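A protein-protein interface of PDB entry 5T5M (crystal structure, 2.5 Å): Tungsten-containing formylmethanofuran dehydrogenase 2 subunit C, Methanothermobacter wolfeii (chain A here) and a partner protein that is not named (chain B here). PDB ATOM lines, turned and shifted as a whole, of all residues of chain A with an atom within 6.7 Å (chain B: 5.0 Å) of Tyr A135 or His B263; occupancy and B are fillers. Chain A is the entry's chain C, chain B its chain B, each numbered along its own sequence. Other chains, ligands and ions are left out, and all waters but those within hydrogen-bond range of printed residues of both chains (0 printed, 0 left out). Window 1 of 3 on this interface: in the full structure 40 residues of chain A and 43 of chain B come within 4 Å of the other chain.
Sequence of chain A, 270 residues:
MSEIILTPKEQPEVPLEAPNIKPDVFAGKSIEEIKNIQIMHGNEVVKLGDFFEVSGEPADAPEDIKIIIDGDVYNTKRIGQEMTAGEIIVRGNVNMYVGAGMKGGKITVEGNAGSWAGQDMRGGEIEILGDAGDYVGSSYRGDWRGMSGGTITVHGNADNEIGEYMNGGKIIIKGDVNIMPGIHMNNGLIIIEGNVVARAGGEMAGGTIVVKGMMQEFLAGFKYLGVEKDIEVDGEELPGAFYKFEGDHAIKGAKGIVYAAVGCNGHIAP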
ATOM      1  N   GLY A 114       5.660 -39.180   0.659  1.00  0.00           N
ATOM      2  CA  GLY A 114       5.807 -37.755   0.820  1.00  0.00           C
ATOM      3  C   GLY A 114       4.560 -36.998   0.402  1.00  0.00           C
ATOM      4  O   GLY A 114       3.481 -37.553   0.194  1.00  0.00           O
ATOM      5  N   SER A 115       4.732 -35.688   0.275  1.00  0.00           N
ATOM      6  CA  SER A 115       3.633 -34.807  -0.077  1.00  0.00           C
ATOM      7  C   SER A 115       3.265 -34.966  -1.548  1.00  0.00           C
ATOM      8  O   SER A 115       4.042 -35.461  -2.365  1.00  0.00           O
ATOM      9  CB  SER A 115       3.995 -33.350   0.219  1.00  0.00           C
ATOM     10  OG  SER A 115       4.019 -33.104   1.617  1.00  0.00           O
ATOM     11  N   TRP A 116       2.036 -34.560  -1.867  1.00  0.00           N
ATOM     12  CA  TRP A 116       1.484 -34.580  -3.227  1.00  0.00           C
ATOM     13  C   TRP A 116       1.300 -35.998  -3.768  1.00  0.00           C
ATOM     14  O   TRP A 116       1.324 -36.215  -4.983  1.00  0.00           O
ATOM     15  CB  TRP A 116       2.330 -33.741  -4.202  1.00  0.00           C
ATOM     16  CG  TRP A 116       2.312 -32.313  -3.833  1.00  0.00           C
ATOM     17  CD1 TRP A 116       1.261 -31.444  -3.955  1.00  0.00           C
ATOM     18  CD2 TRP A 116       3.380 -31.576  -3.242  1.00  0.00           C
ATOM     19  NE1 TRP A 116       1.622 -30.202  -3.487  1.00  0.00           N
ATOM     20  CE2 TRP A 116       2.916 -30.256  -3.040  1.00  0.00           C
ATOM     21  CE3 TRP A 116       4.686 -31.899  -2.873  1.00  0.00           C
ATOM     22  CZ2 TRP A 116       3.718 -29.259  -2.478  1.00  0.00           C
ATOM     23  CZ3 TRP A 116       5.486 -30.907  -2.316  1.00  0.00           C
ATOM     24  CH2 TRP A 116       4.996 -29.600  -2.125  1.00  0.00           C
ATOM     25  N   ALA A 117       1.088 -36.973  -2.891  1.00  0.00           N
ATOM     26  CA  ALA A 117       0.633 -38.284  -3.340  1.00  0.00           C
ATOM     27  C   ALA A 117      -0.699 -38.143  -4.064  1.00  0.00           C
ATOM     28  O   ALA A 117      -1.658 -37.600  -3.509  1.00  0.00           O
ATOM     29  CB  ALA A 117       0.493 -39.228  -2.146  1.00  0.00           C
ATOM     30  N   GLY A 118      -0.757 -38.613  -5.306  1.00  0.00           N
ATOM     31  CA  GLY A 118      -1.995 -38.536  -6.059  1.00  0.00           C
ATOM     32  C   GLY A 118      -2.431 -37.137  -6.430  1.00  0.00           C
ATOM     33  O   GLY A 118      -3.615 -36.907  -6.666  1.00  0.00           O
ATOM     34  N   GLN A 119      -1.504 -36.188  -6.494  1.00  0.00           N
ATOM     35  CA  GLN A 119      -1.827 -34.863  -6.997  1.00  0.00           C
ATOM     36  C   GLN A 119      -2.426 -34.955  -8.395  1.00  0.00           C
ATOM     37  O   GLN A 119      -1.922 -35.679  -9.254  1.00  0.00           O
ATOM     38  CB  GLN A 119      -0.566 -34.001  -7.011  1.00  0.00           C
ATOM     39  CG  GLN A 119      -0.761 -32.581  -7.497  1.00  0.00           C
ATOM     40  CD  GLN A 119       0.550 -31.843  -7.614  1.00  0.00           C
ATOM     41  OE1 GLN A 119       1.538 -32.393  -8.095  1.00  0.00           O
ATOM     42  NE2 GLN A 119       0.575 -30.598  -7.161  1.00  0.00           N
ATOM     43  N   GLY A 133       2.250 -37.234   3.609  1.00  0.00           N
ATOM     44  CA  GLY A 133       2.526 -35.865   3.980  1.00  0.00           C
ATOM     45  C   GLY A 133       1.389 -34.933   3.624  1.00  0.00           C
ATOM     46  O   GLY A 133       0.217 -35.305   3.701  1.00  0.00           O
ATOM     47  N   ASP A 134       1.725 -33.715   3.223  1.00  0.00           N
ATOM     48  CA  ASP A 134       0.708 -32.749   2.865  1.00  0.00           C
ATOM     49  C   ASP A 134       0.180 -33.009   1.454  1.00  0.00           C
ATOM     50  O   ASP A 134       0.808 -33.684   0.634  1.00  0.00           O
ATOM     51  CB  ASP A 134       1.272 -31.334   2.949  1.00  0.00           C
ATOM     52  CG  ASP A 134       1.907 -31.028   4.295  1.00  0.00           C
ATOM     53  OD1 ASP A 134       1.164 -30.892   5.287  1.00  0.00           O
ATOM     54  OD2 ASP A 134       3.149 -30.898   4.359  1.00  0.00           O
ATOM     55  N   TYR A 135      -1.007 -32.473   1.182  1.00  0.00           N
ATOM     56  CA  TYR A 135      -1.511 -32.352  -0.188  1.00  0.00           C
ATOM     57  C   TYR A 135      -1.779 -33.710  -0.829  1.00  0.00           C
ATOM     58  O   TYR A 135      -1.554 -33.896  -2.025  1.00  0.00           O
ATOM     59  CB  TYR A 135      -0.546 -31.545  -1.064  1.00  0.00           C
ATOM     60  CG  TYR A 135      -0.373 -30.111  -0.640  1.00  0.00           C
ATOM     61  CD1 TYR A 135      -1.438 -29.216  -0.688  1.00  0.00           C
ATOM     62  CD2 TYR A 135       0.858 -29.639  -0.209  1.00  0.00           C
ATOM     63  CE1 TYR A 135      -1.282 -27.892  -0.306  1.00  0.00           C
ATOM     64  CE2 TYR A 135       1.023 -28.307   0.171  1.00  0.00           C
ATOM     65  CZ  TYR A 135      -0.053 -27.450   0.119  1.00  0.00           C
ATOM     66  OH  TYR A 135       0.109 -26.153   0.513  1.00  0.00           O
ATOM     67  N   VAL A 136      -2.280 -34.671  -0.044  1.00  0.00           N
ATOM     68  CA  VAL A 136      -2.842 -35.875  -0.648  1.00  0.00           C
ATOM     69  C   VAL A 136      -3.975 -35.456  -1.572  1.00  0.00           C
ATOM     70  O   VAL A 136      -4.916 -34.774  -1.153  1.00  0.00           O
ATOM     71  CB  VAL A 136      -3.332 -36.865   0.419  1.00  0.00           C
ATOM     72  CG1 VAL A 136      -3.768 -38.160  -0.247  1.00  0.00           C
ATOM     73  CG2 VAL A 136      -2.261 -37.173   1.462  1.00  0.00           C
ATOM     74  N   GLY A 137      -3.877 -35.837  -2.840  1.00  0.00           N
ATOM     75  CA  GLY A 137      -4.958 -35.604  -3.792  1.00  0.00           C
ATOM     76  C   GLY A 137      -5.250 -34.142  -4.062  1.00  0.00           C
ATOM     77  O   GLY A 137      -6.417 -33.764  -4.236  1.00  0.00           O
ATOM     78  N   SER A 138      -4.211 -33.312  -4.127  1.00  0.00           N
ATOM     79  CA  SER A 138      -4.380 -31.873  -4.271  1.00  0.00           C
ATOM     80  C   SER A 138      -4.338 -31.448  -5.741  1.00  0.00           C
ATOM     81  O   SER A 138      -4.254 -32.267  -6.662  1.00  0.00           O
ATOM     82  CB  SER A 138      -3.295 -31.138  -3.488  1.00  0.00           C
ATOM     83  OG  SER A 138      -2.029 -31.288  -4.117  1.00  0.00           O
ATOM     84  N   SER A 139      -4.383 -30.137  -5.957  1.00  0.00           N
ATOM     85  CA  SER A 139      -4.124 -29.514  -7.245  1.00  0.00           C
ATOM     86  C   SER A 139      -2.691 -28.993  -7.284  1.00  0.00           C
ATOM     87  O   SER A 139      -1.920 -29.131  -6.331  1.00  0.00           O
ATOM     88  CB  SER A 139      -5.106 -28.373  -7.488  1.00  0.00           C
ATOM     89  OG  SER A 139      -4.839 -27.282  -6.621  1.00  0.00           O
ATOM     90  N   ARG A 141      -0.214 -25.536  -7.758  1.00  0.00           N
ATOM     91  CA  ARG A 141      -0.274 -24.114  -7.439  1.00  0.00           C
ATOM     92  C   ARG A 141      -0.951 -23.326  -8.555  1.00  0.00           C
ATOM     93  O   ARG A 141      -0.606 -23.463  -9.731  1.00  0.00           O
ATOM     94  CB  ARG A 141       1.139 -23.564  -7.208  1.00  0.00           C
ATOM     95  CG  ARG A 141       1.950 -24.282  -6.153  1.00  0.00           C
ATOM     96  CD  ARG A 141       1.255 -24.312  -4.791  1.00  0.00           C
ATOM     97  NE  ARG A 141       2.137 -24.852  -3.761  1.00  0.00           N
ATOM     98  CZ  ARG A 141       1.806 -25.015  -2.485  1.00  0.00           C
ATOM     99  NH1 ARG A 141       0.603 -24.687  -2.037  1.00  0.00           N
ATOM    100  NH2 ARG A 141       2.694 -25.516  -1.649  1.00  0.00           N
ATOM    101  N   ASP A 159      -1.212 -35.165   6.717  1.00  0.00           N
ATOM    102  CA  ASP A 159      -0.974 -33.851   7.315  1.00  0.00           C
ATOM    103  C   ASP A 159      -1.963 -32.781   6.842  1.00  0.00           C
ATOM    104  O   ASP A 159      -3.156 -32.867   7.145  1.00  0.00           O
ATOM    105  CB  ASP A 159       0.476 -33.423   7.047  1.00  0.00           C
ATOM    106  CG  ASP A 159       1.479 -34.263   7.813  1.00  0.00           C
ATOM    107  OD1 ASP A 159       1.172 -34.651   8.960  1.00  0.00           O
ATOM    108  OD2 ASP A 159       2.574 -34.532   7.281  1.00  0.00           O
ATOM    109  N   ASN A 160      -1.488 -31.763   6.120  1.00  0.00           N
ATOM    110  CA  ASN A 160      -2.271 -30.573   5.833  1.00  0.00           C
ATOM    111  C   ASN A 160      -2.865 -30.620   4.437  1.00  0.00           C
ATOM    112  O   ASN A 160      -2.289 -31.195   3.511  1.00  0.00           O
ATOM    113  CB  ASN A 160      -1.417 -29.304   5.943  1.00  0.00           C
ATOM    114  CG  ASN A 160      -1.257 -28.815   7.357  1.00  0.00           C
ATOM    115  OD1 ASN A 160      -1.628 -29.491   8.324  1.00  0.00           O
ATOM    116  ND2 ASN A 160      -0.692 -27.623   7.488  1.00  0.00           N
ATOM    117  N   GLU A 161      -4.017 -29.973   4.290  1.00  0.00           N
ATOM    118  CA  GLU A 161      -4.572 -29.629   2.980  1.00  0.00           C
ATOM    119  C   GLU A 161      -4.764 -30.857   2.105  1.00  0.00           C
ATOM    120  O   GLU A 161      -4.644 -30.779   0.881  1.00  0.00           O
ATOM    121  CB  GLU A 161      -3.696 -28.601   2.252  1.00  0.00           C
ATOM    122  CG  GLU A 161      -3.647 -27.237   2.914  1.00  0.00           C
ATOM    123  CD  GLU A 161      -2.741 -26.266   2.179  1.00  0.00           C
ATOM    124  OE1 GLU A 161      -3.257 -25.491   1.333  1.00  0.00           O
ATOM    125  OE2 GLU A 161      -1.513 -26.294   2.436  1.00  0.00           O
ATOM    126  N   ILE A 162      -5.058 -32.006   2.704  1.00  0.00           N
ATOM    127  CA  ILE A 162      -5.418 -33.149   1.886  1.00  0.00           C
ATOM    128  C   ILE A 162      -6.735 -32.833   1.188  1.00  0.00           C
ATOM    129  O   ILE A 162      -7.646 -32.244   1.782  1.00  0.00           O
ATOM    130  CB  ILE A 162      -5.483 -34.432   2.738  1.00  0.00           C
ATOM    131  CG1 ILE A 162      -6.688 -34.429   3.658  1.00  0.00           C
ATOM    132  CG2 ILE A 162      -4.194 -34.599   3.584  1.00  0.00           C
ATOM    133  CD1 ILE A 162      -7.775 -35.315   3.169  1.00  0.00           C
ATOM    134  N   GLY A 163      -6.820 -33.162  -0.101  1.00  0.00           N
ATOM    135  CA  GLY A 163      -8.006 -32.845  -0.874  1.00  0.00           C
ATOM    136  C   GLY A 163      -8.120 -31.405  -1.334  1.00  0.00           C
ATOM    137  O   GLY A 163      -9.207 -30.980  -1.736  1.00  0.00           O
ATOM    138  N   GLU A 164      -7.023 -30.650  -1.315  1.00  0.00           N
ATOM    139  CA  GLU A 164      -7.036 -29.261  -1.745  1.00  0.00           C
ATOM    140  C   GLU A 164      -7.619 -29.123  -3.148  1.00  0.00           C
ATOM    141  O   GLU A 164      -7.161 -29.771  -4.096  1.00  0.00           O
ATOM    142  CB  GLU A 164      -5.605 -28.715  -1.707  1.00  0.00           C
ATOM    143  CG  GLU A 164      -5.451 -27.254  -2.067  1.00  0.00           C
ATOM    144  CD  GLU A 164      -4.326 -27.018  -3.065  1.00  0.00           C
ATOM    145  OE1 GLU A 164      -4.319 -27.688  -4.120  1.00  0.00           O
ATOM    146  OE2 GLU A 164      -3.441 -26.170  -2.801  1.00  0.00           O
ATOM    147  N   MET A 180      -6.991 -28.246   7.868  1.00  0.00           N
ATOM    148  CA  MET A 180      -7.511 -27.837   6.566  1.00  0.00           C
ATOM    149  C   MET A 180      -7.668 -28.990   5.571  1.00  0.00           C
ATOM    150  O   MET A 180      -7.303 -28.834   4.399  1.00  0.00           O
ATOM    151  CB  MET A 180      -6.602 -26.745   5.979  1.00  0.00           C
ATOM    152  CG  MET A 180      -6.347 -25.602   6.944  1.00  0.00           C
ATOM    153  SD  MET A 180      -5.536 -24.148   6.246  1.00  0.00           S
ATOM    154  CE  MET A 180      -3.896 -24.815   5.896  1.00  0.00           C
ATOM    155  N   ILE A 183      -9.676 -28.089   1.884  1.00  0.00           N
ATOM    156  CA  ILE A 183      -9.618 -26.660   1.615  1.00  0.00           C
ATOM    157  C   ILE A 183      -9.980 -26.421   0.156  1.00  0.00           C
ATOM    158  O   ILE A 183      -9.471 -27.099  -0.746  1.00  0.00           O
ATOM    159  CB  ILE A 183      -8.229 -26.113   1.977  1.00  0.00           C
ATOM    160  CG1 ILE A 183      -8.184 -24.592   1.830  1.00  0.00           C
ATOM    161  CG2 ILE A 183      -7.124 -26.763   1.141  1.00  0.00           C
ATOM    162  CD1 ILE A 183      -8.487 -23.886   3.118  1.00  0.00           C
ATOM    163  N   PRO B 121       4.125 -17.280   1.468  1.00  0.00           N
ATOM    164  CA  PRO B 121       2.722 -17.666   1.693  1.00  0.00           C
ATOM    165  C   PRO B 121       1.742 -16.716   1.026  1.00  0.00           C
ATOM    166  O   PRO B 121       0.692 -17.155   0.539  1.00  0.00           O
ATOM    167  CB  PRO B 121       2.596 -17.655   3.227  1.00  0.00           C
ATOM    168  CG  PRO B 121       3.964 -17.975   3.710  1.00  0.00           C
ATOM    169  CD  PRO B 121       4.898 -17.275   2.726  1.00  0.00           C
ATOM    170  N   LEU B 124       1.811 -17.706  -2.670  1.00  0.00           N
ATOM    171  CA  LEU B 124       0.976 -18.887  -2.876  1.00  0.00           C
ATOM    172  C   LEU B 124      -0.509 -18.540  -2.809  1.00  0.00           C
ATOM    173  O   LEU B 124      -1.310 -19.050  -3.603  1.00  0.00           O
ATOM    174  CB  LEU B 124       1.318 -19.941  -1.832  1.00  0.00           C
ATOM    175  CG  LEU B 124       2.732 -20.510  -1.885  1.00  0.00           C
ATOM    176  CD1 LEU B 124       3.054 -21.272  -0.601  1.00  0.00           C
ATOM    177  CD2 LEU B 124       2.843 -21.407  -3.093  1.00  0.00           C
ATOM    178  N   ALA B 125      -0.897 -17.689  -1.857  1.00  0.00           N
ATOM    179  CA  ALA B 125      -2.291 -17.273  -1.746  1.00  0.00           C
ATOM    180  C   ALA B 125      -2.756 -16.559  -3.010  1.00  0.00           C
ATOM    181  O   ALA B 125      -3.801 -16.905  -3.580  1.00  0.00           O
ATOM    182  CB  ALA B 125      -2.464 -16.367  -0.533  1.00  0.00           C
ATOM    183  N   THR B 257       1.536 -14.774   7.867  1.00  0.00           N
ATOM    184  CA  THR B 257       2.295 -15.659   6.982  1.00  0.00           C
ATOM    185  C   THR B 257       3.052 -16.736   7.751  1.00  0.00           C
ATOM    186  O   THR B 257       3.250 -17.838   7.224  1.00  0.00           O
ATOM    187  CB  THR B 257       3.302 -14.876   6.122  1.00  0.00           C
ATOM    188  OG1 THR B 257       4.336 -14.327   6.942  1.00  0.00           O
ATOM    189  CG2 THR B 257       2.632 -13.758   5.344  1.00  0.00           C
ATOM    190  N   GLY B 261      -1.675 -22.019   9.452  1.00  0.00           N
ATOM    191  CA  GLY B 261      -2.387 -21.921   8.204  1.00  0.00           C
ATOM    192  C   GLY B 261      -1.566 -21.284   7.107  1.00  0.00           C
ATOM    193  O   GLY B 261      -1.763 -21.600   5.922  1.00  0.00           O
ATOM    194  N   LYS B 262      -0.647 -20.394   7.485  1.00  0.00           N
ATOM    195  CA  LYS B 262       0.271 -19.721   6.573  1.00  0.00           C
ATOM    196  C   LYS B 262      -0.446 -19.172   5.343  1.00  0.00           C
ATOM    197  O   LYS B 262      -1.247 -18.239   5.469  1.00  0.00           O
ATOM    198  CB  LYS B 262       1.395 -20.684   6.209  1.00  0.00           C
ATOM    199  CG  LYS B 262       2.194 -21.054   7.462  1.00  0.00           C
ATOM    200  CD  LYS B 262       3.216 -22.145   7.257  1.00  0.00           C
ATOM    201  CE  LYS B 262       3.996 -22.370   8.548  1.00  0.00           C
ATOM    202  NZ  LYS B 262       4.832 -23.588   8.504  1.00  0.00           N
ATOM    203  N   HIS B 263      -0.181 -19.731   4.156  1.00  0.00           N
ATOM    204  CA  HIS B 263      -0.728 -19.145   2.933  1.00  0.00           C
ATOM    205  C   HIS B 263      -2.252 -19.101   2.953  1.00  0.00           C
ATOM    206  O   HIS B 263      -2.852 -18.250   2.289  1.00  0.00           O
ATOM    207  CB  HIS B 263      -0.243 -19.917   1.706  1.00  0.00           C
ATOM    208  CG  HIS B 263      -0.645 -21.353   1.702  1.00  0.00           C
ATOM    209  ND1 HIS B 263      -0.224 -22.246   2.666  1.00  0.00           N
ATOM    210  CD2 HIS B 263      -1.447 -22.050   0.865  1.00  0.00           C
ATOM    211  CE1 HIS B 263      -0.746 -23.433   2.419  1.00  0.00           C
ATOM    212  NE2 HIS B 263      -1.493 -23.340   1.332  1.00  0.00           N
ATOM    213  N   ARG B 264      -2.903 -19.985   3.711  1.00  0.00           N
ATOM    214  CA  ARG B 264      -4.362 -19.957   3.730  1.00  0.00           C
ATOM    215  C   ARG B 264      -4.913 -18.829   4.594  1.00  0.00           C
ATOM    216  O   ARG B 264      -6.069 -18.430   4.402  1.00  0.00           O
ATOM    217  CB  ARG B 264      -4.915 -21.307   4.194  1.00  0.00           C
ATOM    218  CG  ARG B 264      -4.668 -22.464   3.215  1.00  0.00           C
ATOM    219  CD  ARG B 264      -5.204 -22.192   1.795  1.00  0.00           C
ATOM    220  NE  ARG B 264      -4.740 -23.208   0.853  1.00  0.00           N
ATOM    221  CZ  ARG B 264      -4.705 -23.061  -0.470  1.00  0.00           C
ATOM    222  NH1 ARG B 264      -5.128 -21.945  -1.050  1.00  0.00           N
ATOM    223  NH2 ARG B 264      -4.241 -24.046  -1.221  1.00  0.00           N
ATOM    224  N   ASN B 265      -4.110 -18.286   5.515  1.00  0.00           N
ATOM    225  CA  ASN B 265      -4.494 -17.046   6.182  1.00  0.00           C
ATOM    226  C   ASN B 265      -4.550 -15.886   5.189  1.00  0.00           C
ATOM    227  O   ASN B 265      -5.434 -15.021   5.273  1.00  0.00           O
ATOM    228  CB  ASN B 265      -3.513 -16.722   7.304  1.00  0.00           C
ATOM    229  CG  ASN B 265      -3.463 -17.790   8.368  1.00  0.00           C
ATOM    230  OD1 ASN B 265      -4.438 -18.504   8.605  1.00  0.00           O
ATOM    231  ND2 ASN B 265      -2.321 -17.903   9.025  1.00  0.00           N
ATOM    232  N   ILE B 266      -3.615 -15.851   4.234  1.00  0.00           N
ATOM    233  CA  ILE B 266      -3.589 -14.752   3.274  1.00  0.00           C
ATOM    234  C   ILE B 266      -4.691 -14.941   2.247  1.00  0.00           C
ATOM    235  O   ILE B 266      -5.406 -13.996   1.885  1.00  0.00           O
ATOM    236  CB  ILE B 266      -2.217 -14.654   2.588  1.00  0.00           C
ATOM    237  CG1 ILE B 266      -1.068 -14.912   3.576  1.00  0.00           C
ATOM    238  CG2 ILE B 266      -2.103 -13.299   1.889  1.00  0.00           C
ATOM    239  CD1 ILE B 266      -1.055 -14.002   4.785  1.00  0.00           C
ATOM    240  N   ASP B 267      -4.791 -16.160   1.718  1.00  0.00           N
ATOM    241  CA  ASP B 267      -5.915 -16.596   0.905  1.00  0.00           C
ATOM    242  C   ASP B 267      -7.233 -15.982   1.383  1.00  0.00           C
ATOM    243  O   ASP B 267      -7.901 -15.257   0.635  1.00  0.00           O
ATOM    244  CB  ASP B 267      -5.932 -18.129   0.955  1.00  0.00           C
ATOM    245  CG  ASP B 267      -7.083 -18.747   0.228  1.00  0.00           C
ATOM    246  OD1 ASP B 267      -8.218 -18.231   0.332  1.00  0.00           O
ATOM    247  OD2 ASP B 267      -6.850 -19.805  -0.402  1.00  0.00           O
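NE2 of His B263 is in hydrogen-bond range of NE of Arg B264 (3.3 Å). NH1 of Arg B264 lies within salt-bridge range of OD2 of Asp B267 (2.8 Å). OG of Ser A138 is in hydrogen-bond range of O of Tyr A135 (3.4 Å). N of Tyr A135 sits at hydrogen-bond distance from O of Asn A160 (2.9 Å). The side-chain carboxylate (OE2) of Glu A161 lies within hydrogen-bond range of the side-chain hydroxyl (OH) of Tyr A135, 2.5 Å away. N of Ser A139 lies within hydrogen-bond range of OE1 of Glu A164.
The side-chain hydroxyl (OH) of Tyr A135 sits at hydrogen-bond distance from a ring nitrogen (NE2) of His B263. The side-chain carboxylate (OE1) of Glu A161 sits at hydrogen-bond distance from a ring nitrogen (NE2) of His B263, at 2.8 Å. The side-chain carboxylate (OE1) of Glu A161 lies within salt-bridge range of the guanidinium group (NE) of Arg B264 (2.8 Å). NH2 of Arg B264 is in salt-bridge range of OE2 of Glu A164.
Of the 11 printed residues of chain B, 4 touch a printed residue of chain A. Hydrophobic or aromatic side chains of chain B that line the printed part of chain A: Leu B124 and His B263. Hydrophobic or aromatic side chains of chain A within 4 Å of the printed part of chain B: Tyr A135, Met A180 and Ile A183. Among the printed residues, 8 pairs touch across the chains.
Among the printed residues, merely in contact across the chains: Met A180 with Arg B264 (3.6 Å), Arg A141 with Leu B124 (3.6 Å), Ile A183 with Arg B264 (3.8 Å) and Met A180 with Gly B261 (3.9 Å).
Tyr A135 touches just one residue of chain B: His B263 (3.3 Å). Of the printed residues of chain B, Arg A141 touches Leu B124. Of the printed residues of chain A, Leu B124 touches Arg A141 (3.6 Å). Of the printed residues of chain A, His B263 touches Tyr A135 (3.3 Å) and Glu A161 (2.8 Å). Asp B267 touches none of the printed residues of chain A.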
